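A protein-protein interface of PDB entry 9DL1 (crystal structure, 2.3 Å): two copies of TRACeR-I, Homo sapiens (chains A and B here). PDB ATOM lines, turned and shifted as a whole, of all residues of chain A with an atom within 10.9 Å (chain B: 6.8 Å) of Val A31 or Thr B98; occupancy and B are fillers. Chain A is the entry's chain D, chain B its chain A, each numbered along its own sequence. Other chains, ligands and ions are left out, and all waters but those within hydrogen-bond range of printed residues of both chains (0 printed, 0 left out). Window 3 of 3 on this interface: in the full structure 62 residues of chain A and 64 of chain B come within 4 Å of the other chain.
The side-chain carboxylate of Glu A32 lies within salt-bridge range of the side-chain amino group of Lys A35 (3.7 Å).
Among the printed residues, pairs that only touch across the chains: Val A31 with Glu B97 (3.6 Å), Val A31 with Thr B98 (3.5 Å), Ile A34 with Val B101 (3.6 Å), Ile A34 with Leu B102 (3.7 Å) and Lys A35 with Val B101 (3.5 Å).
Asp A27 touches none of the printed residues of chain B. Of chain B, only Glu B97 and Thr B98 come within 4 Å of Val A31. Of the printed residues of chain B, Ile A34 touches Val B101 (3.6 Å) and Leu B102 (3.7 Å). Of the printed residues of chain B, Lys A35 touches Val B101. Lys B95 touches none of the printed residues of chain A. Of chain A, only Val A31 comes within 4 Å of Glu B97. Of chain A, only Val A31 comes within 4 Å of Thr B98. No residue of chain A comes within 4 Å of Lys B99. Leu B102 touches just one residue of chain A: Ile A34 (3.7 Å). The nearest printed residue of chain B that does not touch Ile A34 is Thr B98 (5.3 Å).
Hydrophobic or aromatic side chains of chain A that line the printed part of chain B: Val A31 and Ile A34. Of the 9 printed residues of chain B, 4 touch a printed residue of chain A. Among the printed residues, 5 pairs touch across the chains. Among the printed residues, no Asp or Glu carboxylate lies within 4 Å of a Lys or Arg side-chain nitrogen of the other chain.
No position is printed for both chains. Of the 5 pairs that touch across the chains among the printed residues, none has its exchanged pair printed and touching as well.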
ATOM      1  N   GLN A  24       3.752   3.119  23.036  1.00  0.00           N
ATOM      2  CA  GLN A  24       2.409   2.658  23.377  1.00  0.00           C
ATOM      3  C   GLN A  24       1.430   3.537  22.607  1.00  0.00           C
ATOM      4  O   GLN A  24       1.083   4.650  23.014  1.00  0.00           O
ATOM      5  CB  GLN A  24       2.185   2.679  24.886  1.00  0.00           C
ATOM      6  CG  GLN A  24       0.744   2.873  25.301  1.00  0.00           C
ATOM      7  CD  GLN A  24       0.048   1.561  25.527  1.00  0.00           C
ATOM      8  OE1 GLN A  24       0.198   0.929  26.576  1.00  0.00           O
ATOM      9  NE2 GLN A  24      -0.697   1.111  24.517  1.00  0.00           N
ATOM     10  N   ARG A  25       1.027   3.057  21.437  1.00  0.00           N
ATOM     11  CA  ARG A  25      -0.019   3.727  20.682  1.00  0.00           C
ATOM     12  C   ARG A  25      -1.366   3.393  21.305  1.00  0.00           C
ATOM     13  O   ARG A  25      -1.644   2.229  21.613  1.00  0.00           O
ATOM     14  CB  ARG A  25       0.030   3.305  19.218  1.00  0.00           C
ATOM     15  CG  ARG A  25      -0.725   4.236  18.305  1.00  0.00           C
ATOM     16  CD  ARG A  25      -0.190   4.168  16.882  1.00  0.00           C
ATOM     17  NE  ARG A  25      -1.119   3.483  15.990  1.00  0.00           N
ATOM     18  CZ  ARG A  25      -2.160   4.061  15.406  1.00  0.00           C
ATOM     19  NH1 ARG A  25      -2.451   5.337  15.615  1.00  0.00           N
ATOM     20  NH2 ARG A  25      -2.938   3.337  14.606  1.00  0.00           N
ATOM     21  N   ILE A  26      -2.185   4.417  21.529  1.00  0.00           N
ATOM     22  CA  ILE A  26      -3.484   4.179  22.148  1.00  0.00           C
ATOM     23  C   ILE A  26      -4.546   4.285  21.064  1.00  0.00           C
ATOM     24  O   ILE A  26      -4.977   5.387  20.706  1.00  0.00           O
ATOM     25  CB  ILE A  26      -3.762   5.155  23.313  1.00  0.00           C
ATOM     26  CG1 ILE A  26      -2.940   4.778  24.545  1.00  0.00           C
ATOM     27  CG2 ILE A  26      -5.206   5.096  23.743  1.00  0.00           C
ATOM     28  CD1 ILE A  26      -2.590   5.988  25.398  1.00  0.00           C
ATOM     29  N   ASP A  27      -4.956   3.140  20.525  1.00  0.00           N
ATOM     30  CA  ASP A  27      -6.049   3.062  19.573  1.00  0.00           C
ATOM     31  C   ASP A  27      -7.072   2.043  20.058  1.00  0.00           C
ATOM     32  O   ASP A  27      -6.860   1.334  21.046  1.00  0.00           O
ATOM     33  CB  ASP A  27      -5.541   2.667  18.180  1.00  0.00           C
ATOM     34  CG  ASP A  27      -5.532   3.835  17.211  1.00  0.00           C
ATOM     35  OD1 ASP A  27      -5.705   4.992  17.660  1.00  0.00           O
ATOM     36  OD2 ASP A  27      -5.355   3.592  15.997  1.00  0.00           O
ATOM     37  N   ALA A  28      -8.203   1.989  19.365  1.00  0.00           N
ATOM     38  CA  ALA A  28      -9.030   0.795  19.394  1.00  0.00           C
ATOM     39  C   ALA A  28      -8.427  -0.180  18.394  1.00  0.00           C
ATOM     40  O   ALA A  28      -7.850   0.233  17.380  1.00  0.00           O
ATOM     41  CB  ALA A  28     -10.487   1.111  19.061  1.00  0.00           C
ATOM     42  N   ASN A  29      -8.524  -1.474  18.708  1.00  0.00           N
ATOM     43  CA  ASN A  29      -7.672  -2.525  18.149  1.00  0.00           C
ATOM     44  C   ASN A  29      -6.219  -2.370  18.586  1.00  0.00           C
ATOM     45  O   ASN A  29      -5.342  -3.085  18.081  1.00  0.00           O
ATOM     46  CB  ASN A  29      -7.761  -2.601  16.617  1.00  0.00           C
ATOM     47  CG  ASN A  29      -7.325  -3.952  16.068  1.00  0.00           C
ATOM     48  OD1 ASN A  29      -7.184  -4.929  16.814  1.00  0.00           O
ATOM     49  ND2 ASN A  29      -7.110  -4.013  14.756  1.00  0.00           N
ATOM     50  N   ASN A  30      -5.933  -1.438  19.497  1.00  0.00           N
ATOM     51  CA  ASN A  30      -4.705  -1.450  20.281  1.00  0.00           C
ATOM     52  C   ASN A  30      -4.982  -1.827  21.731  1.00  0.00           C
ATOM     53  O   ASN A  30      -4.122  -1.622  22.594  1.00  0.00           O
ATOM     54  CB  ASN A  30      -3.992  -0.093  20.203  1.00  0.00           C
ATOM     55  CG  ASN A  30      -2.677  -0.160  19.413  1.00  0.00           C
ATOM     56  OD1 ASN A  30      -2.017  -1.202  19.367  1.00  0.00           O
ATOM     57  ND2 ASN A  30      -2.307   0.953  18.777  1.00  0.00           N
ATOM     58  N   VAL A  31      -6.177  -2.360  22.016  1.00  0.00           N
ATOM     59  CA  VAL A  31      -6.518  -2.810  23.361  1.00  0.00           C
ATOM     60  C   VAL A  31      -5.601  -3.944  23.820  1.00  0.00           C
ATOM     61  O   VAL A  31      -5.255  -4.028  25.004  1.00  0.00           O
ATOM     62  CB  VAL A  31      -8.007  -3.211  23.408  1.00  0.00           C
ATOM     63  CG1 VAL A  31      -8.334  -3.974  24.680  1.00  0.00           C
ATOM     64  CG2 VAL A  31      -8.879  -1.973  23.301  1.00  0.00           C
ATOM     65  N   GLU A  32      -5.180  -4.820  22.903  1.00  0.00           N
ATOM     66  CA  GLU A  32      -4.286  -5.907  23.293  1.00  0.00           C
ATOM     67  C   GLU A  32      -2.882  -5.391  23.600  1.00  0.00           C
ATOM     68  O   GLU A  32      -2.221  -5.916  24.501  1.00  0.00           O
ATOM     69  CB  GLU A  32      -4.252  -6.980  22.195  1.00  0.00           C
ATOM     70  CG  GLU A  32      -3.146  -8.040  22.286  1.00  0.00           C
ATOM     71  CD  GLU A  32      -3.157  -8.768  23.626  1.00  0.00           C
ATOM     72  OE1 GLU A  32      -2.128  -8.746  24.360  1.00  0.00           O
ATOM     73  OE2 GLU A  32      -4.251  -9.296  23.966  1.00  0.00           O
ATOM     74  N   LEU A  33      -2.409  -4.366  22.877  1.00  0.00           N
ATOM     75  CA  LEU A  33      -1.127  -3.761  23.233  1.00  0.00           C
ATOM     76  C   LEU A  33      -1.193  -3.146  24.623  1.00  0.00           C
ATOM     77  O   LEU A  33      -0.234  -3.236  25.395  1.00  0.00           O
ATOM     78  CB  LEU A  33      -0.709  -2.710  22.199  1.00  0.00           C
ATOM     79  CG  LEU A  33       0.563  -1.898  22.531  1.00  0.00           C
ATOM     80  CD1 LEU A  33       1.828  -2.756  22.576  1.00  0.00           C
ATOM     81  CD2 LEU A  33       0.777  -0.690  21.606  1.00  0.00           C
ATOM     82  N   ILE A  34      -2.325  -2.539  24.972  1.00  0.00           N
ATOM     83  CA  ILE A  34      -2.453  -1.945  26.297  1.00  0.00           C
ATOM     84  C   ILE A  34      -2.419  -3.022  27.367  1.00  0.00           C
ATOM     85  O   ILE A  34      -1.769  -2.858  28.406  1.00  0.00           O
ATOM     86  CB  ILE A  34      -3.737  -1.101  26.392  1.00  0.00           C
ATOM     87  CG1 ILE A  34      -3.794  -0.082  25.259  1.00  0.00           C
ATOM     88  CG2 ILE A  34      -3.838  -0.429  27.772  1.00  0.00           C
ATOM     89  CD1 ILE A  34      -5.048   0.733  25.251  1.00  0.00           C
ATOM     90  N   LYS A  35      -3.120  -4.134  27.134  1.00  0.00           N
ATOM     91  CA  LYS A  35      -3.120  -5.225  28.099  1.00  0.00           C
ATOM     92  C   LYS A  35      -1.727  -5.822  28.239  1.00  0.00           C
ATOM     93  O   LYS A  35      -1.292  -6.148  29.346  1.00  0.00           O
ATOM     94  CB  LYS A  35      -4.142  -6.286  27.680  1.00  0.00           C
ATOM     95  CG  LYS A  35      -5.598  -5.815  27.793  1.00  0.00           C
ATOM     96  CD  LYS A  35      -6.605  -6.896  27.402  1.00  0.00           C
ATOM     97  CE  LYS A  35      -6.765  -6.975  25.893  1.00  0.00           C
ATOM     98  NZ  LYS A  35      -7.441  -8.237  25.444  1.00  0.00           N
ATOM     99  N   PHE A  36      -1.002  -5.942  27.129  1.00  0.00           N
ATOM    100  CA  PHE A  36       0.387  -6.387  27.191  1.00  0.00           C
ATOM    101  C   PHE A  36       1.251  -5.425  28.020  1.00  0.00           C
ATOM    102  O   PHE A  36       2.098  -5.863  28.811  1.00  0.00           O
ATOM    103  CB  PHE A  36       0.921  -6.563  25.761  1.00  0.00           C
ATOM    104  CG  PHE A  36       2.423  -6.710  25.663  1.00  0.00           C
ATOM    105  CD1 PHE A  36       3.031  -7.937  25.867  1.00  0.00           C
ATOM    106  CD2 PHE A  36       3.225  -5.613  25.339  1.00  0.00           C
ATOM    107  CE1 PHE A  36       4.415  -8.073  25.767  1.00  0.00           C
ATOM    108  CE2 PHE A  36       4.602  -5.745  25.236  1.00  0.00           C
ATOM    109  CZ  PHE A  36       5.192  -6.976  25.454  1.00  0.00           C
ATOM    110  N   ASN A  37       1.038  -4.113  27.883  1.00  0.00           N
ATOM    111  CA  ASN A  37       1.888  -3.167  28.609  1.00  0.00           C
ATOM    112  C   ASN A  37       1.550  -3.088  30.097  1.00  0.00           C
ATOM    113  O   ASN A  37       2.438  -2.821  30.914  1.00  0.00           O
ATOM    114  CB  ASN A  37       1.805  -1.786  27.958  1.00  0.00           C
ATOM    115  CG  ASN A  37       2.576  -1.719  26.649  1.00  0.00           C
ATOM    116  OD1 ASN A  37       3.480  -2.518  26.412  1.00  0.00           O
ATOM    117  ND2 ASN A  37       2.230  -0.767  25.806  1.00  0.00           N
ATOM    118  N   ILE A  38       0.293  -3.328  30.472  1.00  0.00           N
ATOM    119  CA  ILE A  38      -0.034  -3.513  31.883  1.00  0.00           C
ATOM    120  C   ILE A  38       0.785  -4.667  32.467  1.00  0.00           C
ATOM    121  O   ILE A  38       1.369  -4.553  33.551  1.00  0.00           O
ATOM    122  CB  ILE A  38      -1.553  -3.730  32.059  1.00  0.00           C
ATOM    123  CG1 ILE A  38      -2.296  -2.396  32.102  1.00  0.00           C
ATOM    124  CG2 ILE A  38      -1.864  -4.455  33.332  1.00  0.00           C
ATOM    125  CD1 ILE A  38      -3.793  -2.518  31.759  1.00  0.00           C
ATOM    126  N   ARG A  39       0.857  -5.792  31.746  1.00  0.00           N
ATOM    127  CA  ARG A  39       1.681  -6.906  32.217  1.00  0.00           C
ATOM    128  C   ARG A  39       3.168  -6.555  32.234  1.00  0.00           C
ATOM    129  O   ARG A  39       3.901  -7.010  33.123  1.00  0.00           O
ATOM    130  CB  ARG A  39       1.456  -8.144  31.355  1.00  0.00           C
ATOM    131  CG  ARG A  39       0.168  -8.876  31.678  1.00  0.00           C
ATOM    132  CD  ARG A  39      -0.171  -9.867  30.597  1.00  0.00           C
ATOM    133  NE  ARG A  39       0.349 -11.186  30.940  1.00  0.00           N
ATOM    134  CZ  ARG A  39       0.375 -12.222  30.107  1.00  0.00           C
ATOM    135  NH1 ARG A  39      -0.096 -12.125  28.870  1.00  0.00           N
ATOM    136  NH2 ARG A  39       0.894 -13.379  30.522  1.00  0.00           N
ATOM    137  N   LYS B  95     -15.205   0.242  22.297  1.00  0.00           N
ATOM    138  CA  LYS B  95     -15.939   1.292  23.007  1.00  0.00           C
ATOM    139  C   LYS B  95     -15.843   1.123  24.530  1.00  0.00           C
ATOM    140  O   LYS B  95     -14.913   1.625  25.164  1.00  0.00           O
ATOM    141  CB  LYS B  95     -17.412   1.325  22.570  1.00  0.00           C
ATOM    142  CG  LYS B  95     -17.713   0.907  21.120  1.00  0.00           C
ATOM    143  CD  LYS B  95     -16.888   1.719  20.121  1.00  0.00           C
ATOM    144  CE  LYS B  95     -17.498   1.710  18.725  1.00  0.00           C
ATOM    145  NZ  LYS B  95     -16.714   2.576  17.803  1.00  0.00           N
ATOM    146  N   GLU B  96     -16.818   0.429  25.121  1.00  0.00           N
ATOM    147  CA  GLU B  96     -16.757   0.142  26.551  1.00  0.00           C
ATOM    148  C   GLU B  96     -15.543  -0.710  26.900  1.00  0.00           C
ATOM    149  O   GLU B  96     -14.955  -0.544  27.976  1.00  0.00           O
ATOM    150  CB  GLU B  96     -18.043  -0.554  26.997  1.00  0.00           C
ATOM    151  CG  GLU B  96     -19.274   0.337  26.949  1.00  0.00           C
ATOM    152  CD  GLU B  96     -19.148   1.568  27.838  1.00  0.00           C
ATOM    153  OE1 GLU B  96     -18.855   1.409  29.046  1.00  0.00           O
ATOM    154  OE2 GLU B  96     -19.339   2.695  27.332  1.00  0.00           O
ATOM    155  N   GLU B  97     -15.151  -1.619  26.005  1.00  0.00           N
ATOM    156  CA  GLU B  97     -13.960  -2.429  26.244  1.00  0.00           C
ATOM    157  C   GLU B  97     -12.698  -1.567  26.297  1.00  0.00           C
ATOM    158  O   GLU B  97     -11.842  -1.763  27.168  1.00  0.00           O
ATOM    159  CB  GLU B  97     -13.854  -3.516  25.166  1.00  0.00           C
ATOM    160  CG  GLU B  97     -12.451  -3.770  24.630  1.00  0.00           C
ATOM    161  CD  GLU B  97     -12.361  -5.032  23.783  1.00  0.00           C
ATOM    162  OE1 GLU B  97     -13.297  -5.291  22.992  1.00  0.00           O
ATOM    163  OE2 GLU B  97     -11.348  -5.760  23.907  1.00  0.00           O
ATOM    164  N   THR B  98     -12.578  -0.592  25.393  1.00  0.00           N
ATOM    165  CA  THR B  98     -11.388   0.255  25.355  1.00  0.00           C
ATOM    166  C   THR B  98     -11.292   1.155  26.585  1.00  0.00           C
ATOM    167  O   THR B  98     -10.225   1.274  27.199  1.00  0.00           O
ATOM    168  CB  THR B  98     -11.380   1.096  24.080  1.00  0.00           C
ATOM    169  OG1 THR B  98     -11.608   0.252  22.945  1.00  0.00           O
ATOM    170  CG2 THR B  98     -10.059   1.823  23.924  1.00  0.00           C
ATOM    171  N   LYS B  99     -12.395   1.807  26.957  1.00  0.00           N
ATOM    172  CA  LYS B  99     -12.368   2.652  28.145  1.00  0.00           C
ATOM    173  C   LYS B  99     -12.087   1.846  29.411  1.00  0.00           C
ATOM    174  O   LYS B  99     -11.649   2.420  30.414  1.00  0.00           O
ATOM    175  CB  LYS B  99     -13.689   3.424  28.284  1.00  0.00           C
ATOM    176  CG  LYS B  99     -13.794   4.722  27.430  1.00  0.00           C
ATOM    177  CD  LYS B  99     -12.607   5.707  27.555  1.00  0.00           C
ATOM    178  CE  LYS B  99     -12.161   6.000  29.002  1.00  0.00           C
ATOM    179  NZ  LYS B  99     -11.024   6.984  29.037  1.00  0.00           N
ATOM    180  N   GLU B 100     -12.303   0.524  29.378  1.00  0.00           N
ATOM    181  CA  GLU B 100     -12.067  -0.299  30.559  1.00  0.00           C
ATOM    182  C   GLU B 100     -10.595  -0.679  30.707  1.00  0.00           C
ATOM    183  O   GLU B 100     -10.075  -0.749  31.828  1.00  0.00           O
ATOM    184  CB  GLU B 100     -12.948  -1.547  30.505  1.00  0.00           C
ATOM    185  CG  GLU B 100     -12.990  -2.341  31.801  1.00  0.00           C
ATOM    186  CD  GLU B 100     -13.288  -1.475  33.017  1.00  0.00           C
ATOM    187  OE1 GLU B 100     -13.957  -0.420  32.879  1.00  0.00           O
ATOM    188  OE2 GLU B 100     -12.852  -1.859  34.125  1.00  0.00           O
ATOM    189  N   VAL B 101      -9.905  -0.938  29.597  1.00  0.00           N
ATOM    190  CA  VAL B 101      -8.471  -1.166  29.693  1.00  0.00           C
ATOM    191  C   VAL B 101      -7.760   0.130  30.061  1.00  0.00           C
ATOM    192  O   VAL B 101      -6.810   0.130  30.849  1.00  0.00           O
ATOM    193  CB  VAL B 101      -7.938  -1.794  28.386  1.00  0.00           C
ATOM    194  CG1 VAL B 101      -7.698  -0.762  27.307  1.00  0.00           C
ATOM    195  CG2 VAL B 101      -6.663  -2.545  28.655  1.00  0.00           C
ATOM    196  N   LEU B 102      -8.244   1.256  29.534  1.00  0.00           N
ATOM    197  CA  LEU B 102      -7.654   2.551  29.855  1.00  0.00           C
ATOM    198  C   LEU B 102      -7.773   2.843  31.344  1.00  0.00           C
ATOM    199  O   LEU B 102      -6.816   3.312  31.979  1.00  0.00           O
ATOM    200  CB  LEU B 102      -8.332   3.645  29.025  1.00  0.00           C
ATOM    201  CG  LEU B 102      -7.920   3.622  27.550  1.00  0.00           C
ATOM    202  CD1 LEU B 102      -8.283   4.906  26.840  1.00  0.00           C
ATOM    203  CD2 LEU B 102      -6.436   3.350  27.401  1.00  0.00           C
ATOM    204  N   LYS B 103      -8.932   2.545  31.926  1.00  0.00           N
ATOM    205  CA  LYS B 103      -9.076   2.707  33.362  1.00  0.00           C
ATOM    206  C   LYS B 103      -8.117   1.784  34.111  1.00  0.00           C
ATOM    207  O   LYS B 103      -7.457   2.213  35.064  1.00  0.00           O
ATOM    208  CB  LYS B 103     -10.527   2.456  33.764  1.00  0.00           C
ATOM    209  CG  LYS B 103     -10.810   2.666  35.235  1.00  0.00           C
ATOM    210  CD  LYS B 103     -12.067   1.946  35.656  1.00  0.00           C
ATOM    211  CE  LYS B 103     -12.393   2.230  37.113  1.00  0.00           C
ATOM    212  NZ  LYS B 103     -13.253   1.153  37.681  1.00  0.00           N
